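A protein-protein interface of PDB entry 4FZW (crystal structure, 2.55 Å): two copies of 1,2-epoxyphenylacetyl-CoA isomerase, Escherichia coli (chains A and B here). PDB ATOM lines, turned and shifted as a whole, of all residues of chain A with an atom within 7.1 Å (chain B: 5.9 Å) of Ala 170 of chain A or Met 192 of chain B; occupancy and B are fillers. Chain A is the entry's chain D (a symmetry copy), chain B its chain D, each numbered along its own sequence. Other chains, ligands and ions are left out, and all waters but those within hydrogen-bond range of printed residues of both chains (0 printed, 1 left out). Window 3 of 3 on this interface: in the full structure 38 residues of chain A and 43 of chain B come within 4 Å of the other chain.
Positions printed for both chains: 167 and 175. Of the 14 pairs that touch across the chains among the printed residues, none has its exchanged pair printed and touching as well.
Printed residues of chain B within 4 Å of Gly 168 of chain A: Arg 165 (3.7 Å). Printed residues of chain B within 4 Å of Ala 170 of chain A: Val 166, Gly 191, Met 192 and Trp 194. Of the printed residues of chain B, Gly 174 of chain A touches Trp 194. Of the printed residues of chain B, Leu 175 of chain A touches Trp 194 (3.6 Å). Printed residues of chain A within 4 Å of Arg 165 of chain B: Gly 168 and Arg 169. Printed residues of chain A within 4 Å of Trp 190 of chain B: Arg 171. Gly 191 of chain B touches two residues of chain A. Of the printed residues of chain A, Met 192 of chain B touches Ala 170. The nearest printed residue of chain B that does not touch Ala 170 of chain A is Ile 193 of chain B (4.2 Å). The nearest printed residue of chain B that does not touch Gly 168 of chain A is Val 166 of chain B (5.5 Å).
O of Val 136 of chain B sits at hydrogen-bond distance from N of Trp 194 of chain B (2.9 Å). NE2 of Gln 186 of chain B sits close to NE1 of Trp 190 of chain B (2.8 Å). The backbone NH of Met 192 of chain B lies within hydrogen-bond range of the backbone carbonyl oxygen of Ala 187 of chain B, 3.1 Å away.
Hydrophobic or aromatic side chains of chain B within 4 Å of the printed part of chain A: Val 166 and Trp 194. Of the 10 printed residues of chain A, 7 touch a printed residue of chain B. Hydrophobic or aromatic side chains of chain A within 4 Å of the printed part of chain B: Ala 170 and Met 173. Among the printed residues, no Asp or Glu carboxylate lies within 4 Å of a Lys or Arg side-chain nitrogen of the other chain.
Among the printed residues, pairs that only touch across the chains: Ala 170 of chain A with Gly 191 of chain B (3.3 Å), Gly 174 of chain A with Trp 194 of chain B (3.4 Å), Ala 170 of chain A with Met 192 of chain B (3.4 Å), Met 173 of chain A with Asp 134 of chain B (3.4 Å), Leu 175 of chain A with Trp 194 of chain B (3.6 Å), Arg 171 of chain A with Trp 194 of chain B (3.6 Å), Arg 171 of chain A with Trp 190 of chain B (3.6 Å), Gly 168 of chain A with Arg 165 of chain B (3.7 Å), Arg 171 of chain A with His 188 of chain B (3.8 Å), Ala 170 of chain A with Trp 194 of chain B (3.9 Å) and Ala 170 of chain A with Val 166 of chain B (3.996 Å).
The backbone carbonyl oxygen (O) of Arg 165 of chain B sits at hydrogen-bond distance from the backbone NH (N) of Arg 169 of chain A, at 2.8 Å. NH2 of Arg 171 of chain A sits at hydrogen-bond distance from O of Glu 189 of chain B (3.4 Å). The guanidinium group (NH2) of Arg 171 of chain A lies close to the backbone NH (N) of Gly 191 of chain B, 3.1 Å away.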
ATOM      1  N   PRO A 164      21.055   9.990   0.614  1.00  0.00           N
ATOM      2  CA  PRO A 164      22.288  10.154   1.394  1.00  0.00           C
ATOM      3  C   PRO A 164      23.469   9.417   0.759  1.00  0.00           C
ATOM      4  O   PRO A 164      24.608   9.835   0.901  1.00  0.00           O
ATOM      5  CB  PRO A 164      21.928   9.541   2.769  1.00  0.00           C
ATOM      6  CG  PRO A 164      20.436   9.555   2.816  1.00  0.00           C
ATOM      7  CD  PRO A 164      20.031   9.267   1.385  1.00  0.00           C
ATOM      8  N   ALA A 167      23.991  11.288  -3.116  1.00  0.00           N
ATOM      9  CA  ALA A 167      24.389  12.698  -3.051  1.00  0.00           C
ATOM     10  C   ALA A 167      25.232  13.027  -1.827  1.00  0.00           C
ATOM     11  O   ALA A 167      25.766  14.114  -1.726  1.00  0.00           O
ATOM     12  CB  ALA A 167      23.151  13.598  -3.083  1.00  0.00           C
ATOM     13  N   GLY A 168      25.340  12.092  -0.891  1.00  0.00           N
ATOM     14  CA  GLY A 168      25.978  12.366   0.386  1.00  0.00           C
ATOM     15  C   GLY A 168      24.986  13.048   1.306  1.00  0.00           C
ATOM     16  O   GLY A 168      23.915  13.465   0.859  1.00  0.00           O
ATOM     17  N   ARG A 169      25.340  13.179   2.585  1.00  0.00           N
ATOM     18  CA  ARG A 169      24.375  13.579   3.617  1.00  0.00           C
ATOM     19  C   ARG A 169      23.876  15.027   3.583  1.00  0.00           C
ATOM     20  O   ARG A 169      22.660  15.262   3.689  1.00  0.00           O
ATOM     21  CB  ARG A 169      24.855  13.202   5.034  1.00  0.00           C
ATOM     22  CG  ARG A 169      24.154  13.996   6.129  1.00  0.00           C
ATOM     23  CD  ARG A 169      24.607  13.621   7.529  1.00  0.00           C
ATOM     24  NE  ARG A 169      23.601  12.814   8.210  1.00  0.00           N
ATOM     25  CZ  ARG A 169      22.700  13.293   9.059  1.00  0.00           C
ATOM     26  NH1 ARG A 169      22.680  14.585   9.361  1.00  0.00           N
ATOM     27  NH2 ARG A 169      21.827  12.473   9.616  1.00  0.00           N
ATOM     28  N   ALA A 170      24.789  15.995   3.444  1.00  0.00           N
ATOM     29  CA  ALA A 170      24.377  17.401   3.524  1.00  0.00           C
ATOM     30  C   ALA A 170      23.447  17.742   2.367  1.00  0.00           C
ATOM     31  O   ALA A 170      22.547  18.577   2.498  1.00  0.00           O
ATOM     32  CB  ALA A 170      25.586  18.347   3.562  1.00  0.00           C
ATOM     33  N   ARG A 171      23.643  17.066   1.241  1.00  0.00           N
ATOM     34  CA  ARG A 171      22.878  17.395   0.046  1.00  0.00           C
ATOM     35  C   ARG A 171      21.531  16.689   0.032  1.00  0.00           C
ATOM     36  O   ARG A 171      20.523  17.293  -0.327  1.00  0.00           O
ATOM     37  CB  ARG A 171      23.707  17.144  -1.220  1.00  0.00           C
ATOM     38  CG  ARG A 171      25.015  17.991  -1.218  1.00  0.00           C
ATOM     39  CD  ARG A 171      25.576  18.267  -2.618  1.00  0.00           C
ATOM     40  NE  ARG A 171      27.029  18.127  -2.655  1.00  0.00           N
ATOM     41  CZ  ARG A 171      27.820  18.654  -3.587  1.00  0.00           C
ATOM     42  NH1 ARG A 171      27.308  19.390  -4.547  1.00  0.00           N
ATOM     43  NH2 ARG A 171      29.129  18.456  -3.551  1.00  0.00           N
ATOM     44  N   ALA A 172      21.508  15.423   0.448  1.00  0.00           N
ATOM     45  CA  ALA A 172      20.246  14.682   0.635  1.00  0.00           C
ATOM     46  C   ALA A 172      19.305  15.438   1.557  1.00  0.00           C
ATOM     47  O   ALA A 172      18.114  15.539   1.294  1.00  0.00           O
ATOM     48  CB  ALA A 172      20.499  13.275   1.198  1.00  0.00           C
ATOM     49  N   MET A 173      19.860  15.984   2.631  1.00  0.00           N
ATOM     50  CA  MET A 173      19.056  16.707   3.600  1.00  0.00           C
ATOM     51  C   MET A 173      18.509  17.997   2.953  1.00  0.00           C
ATOM     52  O   MET A 173      17.295  18.199   2.896  1.00  0.00           O
ATOM     53  CB  MET A 173      19.864  16.962   4.878  1.00  0.00           C
ATOM     54  CG  MET A 173      19.054  17.283   6.102  1.00  0.00           C
ATOM     55  SD  MET A 173      18.012  15.930   6.687  1.00  0.00           S
ATOM     56  CE  MET A 173      19.034  15.290   8.026  1.00  0.00           C
ATOM     57  N   GLY A 174      19.407  18.826   2.418  1.00  0.00           N
ATOM     58  CA  GLY A 174      19.054  19.978   1.592  1.00  0.00           C
ATOM     59  C   GLY A 174      18.009  19.711   0.513  1.00  0.00           C
ATOM     60  O   GLY A 174      17.046  20.460   0.409  1.00  0.00           O
ATOM     61  N   LEU A 175      18.185  18.658  -0.287  1.00  0.00           N
ATOM     62  CA  LEU A 175      17.207  18.319  -1.334  1.00  0.00           C
ATOM     63  C   LEU A 175      15.855  17.928  -0.777  1.00  0.00           C
ATOM     64  O   LEU A 175      14.820  18.280  -1.338  1.00  0.00           O
ATOM     65  CB  LEU A 175      17.703  17.189  -2.246  1.00  0.00           C
ATOM     66  CG  LEU A 175      18.872  17.581  -3.144  1.00  0.00           C
ATOM     67  CD1 LEU A 175      19.463  16.380  -3.865  1.00  0.00           C
ATOM     68  CD2 LEU A 175      18.470  18.676  -4.133  1.00  0.00           C
ATOM     69  N   LEU B 131      28.897  21.508  11.297  1.00  0.00           N
ATOM     70  CA  LEU B 131      28.780  20.604  10.160  1.00  0.00           C
ATOM     71  C   LEU B 131      27.596  19.664  10.341  1.00  0.00           C
ATOM     72  O   LEU B 131      27.150  19.020   9.384  1.00  0.00           O
ATOM     73  CB  LEU B 131      30.075  19.806   9.975  1.00  0.00           C
ATOM     74  CG  LEU B 131      31.173  20.558   9.216  1.00  0.00           C
ATOM     75  CD1 LEU B 131      32.501  19.793   9.116  1.00  0.00           C
ATOM     76  CD2 LEU B 131      30.661  20.910   7.833  1.00  0.00           C
ATOM     77  N   ASP B 134      21.330  20.542   9.811  1.00  0.00           N
ATOM     78  CA  ASP B 134      20.579  19.992   8.683  1.00  0.00           C
ATOM     79  C   ASP B 134      20.858  20.748   7.408  1.00  0.00           C
ATOM     80  O   ASP B 134      20.922  20.166   6.318  1.00  0.00           O
ATOM     81  CB  ASP B 134      19.093  20.055   8.994  1.00  0.00           C
ATOM     82  CG  ASP B 134      18.790  19.510  10.357  1.00  0.00           C
ATOM     83  OD1 ASP B 134      19.446  18.513  10.736  1.00  0.00           O
ATOM     84  OD2 ASP B 134      17.928  20.084  11.053  1.00  0.00           O
ATOM     85  N   VAL B 136      23.473  23.968   6.214  1.00  0.00           N
ATOM     86  CA  VAL B 136      24.563  24.843   6.601  1.00  0.00           C
ATOM     87  C   VAL B 136      24.878  25.872   5.503  1.00  0.00           C
ATOM     88  O   VAL B 136      25.163  25.526   4.359  1.00  0.00           O
ATOM     89  CB  VAL B 136      25.823  24.038   6.957  1.00  0.00           C
ATOM     90  CG1 VAL B 136      26.939  24.966   7.428  1.00  0.00           C
ATOM     91  CG2 VAL B 136      25.505  23.003   8.011  1.00  0.00           C
ATOM     92  N   MET B 146      39.405  21.654  11.779  1.00  0.00           N
ATOM     93  CA  MET B 146      39.368  20.479  12.636  1.00  0.00           C
ATOM     94  C   MET B 146      40.779  19.966  12.877  1.00  0.00           C
ATOM     95  O   MET B 146      41.226  19.011  12.232  1.00  0.00           O
ATOM     96  CB  MET B 146      38.501  19.380  12.023  1.00  0.00           C
ATOM     97  CG  MET B 146      37.034  19.746  11.946  1.00  0.00           C
ATOM     98  SD  MET B 146      36.112  18.675  10.817  1.00  0.00           S
ATOM     99  CE  MET B 146      36.878  19.088   9.238  1.00  0.00           C
ATOM    100  N   LEU B 163      31.752  13.154   9.146  1.00  0.00           N
ATOM    101  CA  LEU B 163      32.677  13.478   8.050  1.00  0.00           C
ATOM    102  C   LEU B 163      32.565  12.515   6.884  1.00  0.00           C
ATOM    103  O   LEU B 163      32.584  12.960   5.730  1.00  0.00           O
ATOM    104  CB  LEU B 163      34.132  13.596   8.513  1.00  0.00           C
ATOM    105  CG  LEU B 163      34.393  14.773   9.449  1.00  0.00           C
ATOM    106  CD1 LEU B 163      35.808  14.721  10.003  1.00  0.00           C
ATOM    107  CD2 LEU B 163      34.143  16.062   8.705  1.00  0.00           C
ATOM    108  N   ARG B 165      30.025  10.809   5.896  1.00  0.00           N
ATOM    109  CA  ARG B 165      28.719  10.971   5.265  1.00  0.00           C
ATOM    110  C   ARG B 165      28.576  12.329   4.521  1.00  0.00           C
ATOM    111  O   ARG B 165      27.917  12.445   3.483  1.00  0.00           O
ATOM    112  CB  ARG B 165      27.648  10.807   6.354  1.00  0.00           C
ATOM    113  CG  ARG B 165      27.782   9.488   7.096  1.00  0.00           C
ATOM    114  CD  ARG B 165      26.690   9.211   8.136  1.00  0.00           C
ATOM    115  NE  ARG B 165      26.499   7.764   8.230  1.00  0.00           N
ATOM    116  CZ  ARG B 165      27.263   6.929   8.927  1.00  0.00           C
ATOM    117  NH1 ARG B 165      28.287   7.352   9.663  1.00  0.00           N
ATOM    118  NH2 ARG B 165      26.977   5.645   8.890  1.00  0.00           N
ATOM    119  N   VAL B 166      29.233  13.346   5.049  1.00  0.00           N
ATOM    120  CA  VAL B 166      29.109  14.681   4.509  1.00  0.00           C
ATOM    121  C   VAL B 166      30.141  14.923   3.391  1.00  0.00           C
ATOM    122  O   VAL B 166      29.864  15.630   2.427  1.00  0.00           O
ATOM    123  CB  VAL B 166      29.157  15.726   5.660  1.00  0.00           C
ATOM    124  CG1 VAL B 166      29.880  16.955   5.249  1.00  0.00           C
ATOM    125  CG2 VAL B 166      27.744  16.053   6.134  1.00  0.00           C
ATOM    126  N   ALA B 167      31.310  14.289   3.512  1.00  0.00           N
ATOM    127  CA  ALA B 167      32.419  14.463   2.567  1.00  0.00           C
ATOM    128  C   ALA B 167      32.786  13.183   1.830  1.00  0.00           C
ATOM    129  O   ALA B 167      33.574  13.214   0.905  1.00  0.00           O
ATOM    130  CB  ALA B 167      33.649  15.012   3.295  1.00  0.00           C
ATOM    131  N   LEU B 175      40.779  14.808   5.977  1.00  0.00           N
ATOM    132  CA  LEU B 175      40.509  15.952   6.863  1.00  0.00           C
ATOM    133  C   LEU B 175      40.838  15.669   8.313  1.00  0.00           C
ATOM    134  O   LEU B 175      41.347  16.535   9.021  1.00  0.00           O
ATOM    135  CB  LEU B 175      39.050  16.418   6.777  1.00  0.00           C
ATOM    136  CG  LEU B 175      38.681  17.068   5.447  1.00  0.00           C
ATOM    137  CD1 LEU B 175      37.186  17.315   5.330  1.00  0.00           C
ATOM    138  CD2 LEU B 175      39.473  18.356   5.219  1.00  0.00           C
ATOM    139  N   LEU B 182      39.799  24.114   6.123  1.00  0.00           N
ATOM    140  CA  LEU B 182      38.909  23.848   5.024  1.00  0.00           C
ATOM    141  C   LEU B 182      38.135  25.147   4.887  1.00  0.00           C
ATOM    142  O   LEU B 182      37.492  25.604   5.828  1.00  0.00           O
ATOM    143  CB  LEU B 182      37.977  22.695   5.413  1.00  0.00           C
ATOM    144  CG  LEU B 182      36.964  22.115   4.420  1.00  0.00           C
ATOM    145  CD1 LEU B 182      37.627  21.341   3.305  1.00  0.00           C
ATOM    146  CD2 LEU B 182      35.978  21.222   5.143  1.00  0.00           C
ATOM    147  N   GLN B 186      35.705  25.369  -0.351  1.00  0.00           N
ATOM    148  CA  GLN B 186      36.156  24.003  -0.444  1.00  0.00           C
ATOM    149  C   GLN B 186      35.073  23.074   0.114  1.00  0.00           C
ATOM    150  O   GLN B 186      34.627  22.132  -0.546  1.00  0.00           O
ATOM    151  CB  GLN B 186      37.453  23.828   0.336  1.00  0.00           C
ATOM    152  CG  GLN B 186      38.178  22.555  -0.018  1.00  0.00           C
ATOM    153  CD  GLN B 186      38.571  22.520  -1.480  1.00  0.00           C
ATOM    154  OE1 GLN B 186      39.359  23.339  -1.932  1.00  0.00           O
ATOM    155  NE2 GLN B 186      38.013  21.577  -2.227  1.00  0.00           N
ATOM    156  N   ALA B 187      34.644  23.359   1.338  1.00  0.00           N
ATOM    157  CA  ALA B 187      33.614  22.581   1.981  1.00  0.00           C
ATOM    158  C   ALA B 187      32.430  22.445   1.016  1.00  0.00           C
ATOM    159  O   ALA B 187      31.905  21.345   0.794  1.00  0.00           O
ATOM    160  CB  ALA B 187      33.197  23.265   3.240  1.00  0.00           C
ATOM    161  N   HIS B 188      32.029  23.563   0.418  1.00  0.00           N
ATOM    162  CA  HIS B 188      30.894  23.570  -0.504  1.00  0.00           C
ATOM    163  C   HIS B 188      31.138  22.601  -1.676  1.00  0.00           C
ATOM    164  O   HIS B 188      30.372  21.660  -1.892  1.00  0.00           O
ATOM    165  CB  HIS B 188      30.601  25.000  -0.990  1.00  0.00           C
ATOM    166  CG  HIS B 188      29.399  25.102  -1.876  1.00  0.00           C
ATOM    167  ND1 HIS B 188      28.169  24.584  -1.539  1.00  0.00           N
ATOM    168  CD2 HIS B 188      29.238  25.669  -3.098  1.00  0.00           C
ATOM    169  CE1 HIS B 188      27.304  24.812  -2.512  1.00  0.00           C
ATOM    170  NE2 HIS B 188      27.931  25.466  -3.468  1.00  0.00           N
ATOM    171  N   GLU B 189      32.224  22.838  -2.407  1.00  0.00           N
ATOM    172  CA  GLU B 189      32.588  22.054  -3.581  1.00  0.00           C
ATOM    173  C   GLU B 189      32.576  20.583  -3.220  1.00  0.00           C
ATOM    174  O   GLU B 189      32.246  19.731  -4.044  1.00  0.00           O
ATOM    175  CB  GLU B 189      33.972  22.495  -4.090  1.00  0.00           C
ATOM    176  CG  GLU B 189      34.522  21.754  -5.318  1.00  0.00           C
ATOM    177  CD  GLU B 189      36.014  22.034  -5.545  1.00  0.00           C
ATOM    178  OE1 GLU B 189      36.833  21.080  -5.586  1.00  0.00           O
ATOM    179  OE2 GLU B 189      36.365  23.228  -5.669  1.00  0.00           O
ATOM    180  N   TRP B 190      32.926  20.306  -1.969  1.00  0.00           N
ATOM    181  CA  TRP B 190      33.051  18.953  -1.457  1.00  0.00           C
ATOM    182  C   TRP B 190      31.712  18.322  -1.000  1.00  0.00           C
ATOM    183  O   TRP B 190      31.619  17.106  -0.739  1.00  0.00           O
ATOM    184  CB  TRP B 190      34.081  18.962  -0.333  1.00  0.00           C
ATOM    185  CG  TRP B 190      35.500  18.893  -0.826  1.00  0.00           C
ATOM    186  CD1 TRP B 190      35.926  19.080  -2.111  1.00  0.00           C
ATOM    187  CD2 TRP B 190      36.679  18.584  -0.057  1.00  0.00           C
ATOM    188  NE1 TRP B 190      37.291  18.912  -2.193  1.00  0.00           N
ATOM    189  CE2 TRP B 190      37.777  18.606  -0.948  1.00  0.00           C
ATOM    190  CE3 TRP B 190      36.911  18.280   1.291  1.00  0.00           C
ATOM    191  CZ2 TRP B 190      39.091  18.339  -0.532  1.00  0.00           C
ATOM    192  CZ3 TRP B 190      38.217  18.019   1.700  1.00  0.00           C
ATOM    193  CH2 TRP B 190      39.289  18.059   0.788  1.00  0.00           C
ATOM    194  N   GLY B 191      30.669  19.137  -0.907  1.00  0.00           N
ATOM    195  CA  GLY B 191      29.349  18.609  -0.586  1.00  0.00           C
ATOM    196  C   GLY B 191      29.026  18.588   0.902  1.00  0.00           C
ATOM    197  O   GLY B 191      27.989  18.099   1.314  1.00  0.00           O
ATOM    198  N   MET B 192      29.916  19.180   1.692  1.00  0.00           N
ATOM    199  CA  MET B 192      29.837  19.170   3.139  1.00  0.00           C
ATOM    200  C   MET B 192      28.832  20.171   3.694  1.00  0.00           C
ATOM    201  O   MET B 192      28.319  20.007   4.815  1.00  0.00           O
ATOM    202  CB  MET B 192      31.229  19.434   3.716  1.00  0.00           C
ATOM    203  CG  MET B 192      32.269  18.465   3.186  1.00  0.00           C
ATOM    204  SD  MET B 192      33.931  18.722   3.835  1.00  0.00           S
ATOM    205  CE  MET B 192      33.559  19.033   5.547  1.00  0.00           C
ATOM    206  N   ILE B 193      28.564  21.216   2.918  1.00  0.00           N
ATOM    207  CA  ILE B 193      27.585  22.221   3.313  1.00  0.00           C
ATOM    208  C   ILE B 193      26.689  22.621   2.157  1.00  0.00           C
ATOM    209  O   ILE B 193      26.956  22.288   1.000  1.00  0.00           O
ATOM    210  CB  ILE B 193      28.234  23.469   3.933  1.00  0.00           C
ATOM    211  CG1 ILE B 193      29.111  24.212   2.911  1.00  0.00           C
ATOM    212  CG2 ILE B 193      29.050  23.088   5.145  1.00  0.00           C
ATOM    213  CD1 ILE B 193      29.739  25.441   3.484  1.00  0.00           C
ATOM    214  N   TRP B 194      25.621  23.337   2.476  1.00  0.00           N
ATOM    215  CA  TRP B 194      24.590  23.583   1.489  1.00  0.00           C
ATOM    216  C   TRP B 194      24.856  24.842   0.634  1.00  0.00           C
ATOM    217  O   TRP B 194      24.609  24.842  -0.575  1.00  0.00           O
ATOM    218  CB  TRP B 194      23.229  23.647   2.171  1.00  0.00           C
ATOM    219  CG  TRP B 194      22.090  23.815   1.229  1.00  0.00           C
ATOM    220  CD1 TRP B 194      21.334  24.937   1.049  1.00  0.00           C
ATOM    221  CD2 TRP B 194      21.563  22.824   0.334  1.00  0.00           C
ATOM    222  NE1 TRP B 194      20.373  24.711   0.096  1.00  0.00           N
ATOM    223  CE2 TRP B 194      20.489  23.422  -0.361  1.00  0.00           C
ATOM    224  CE3 TRP B 194      21.897  21.496   0.050  1.00  0.00           C
ATOM    225  CZ2 TRP B 194      19.738  22.733  -1.318  1.00  0.00           C
ATOM    226  CZ3 TRP B 194      21.146  20.810  -0.910  1.00  0.00           C
ATOM    227  CH2 TRP B 194      20.077  21.431  -1.574  1.00  0.00           C
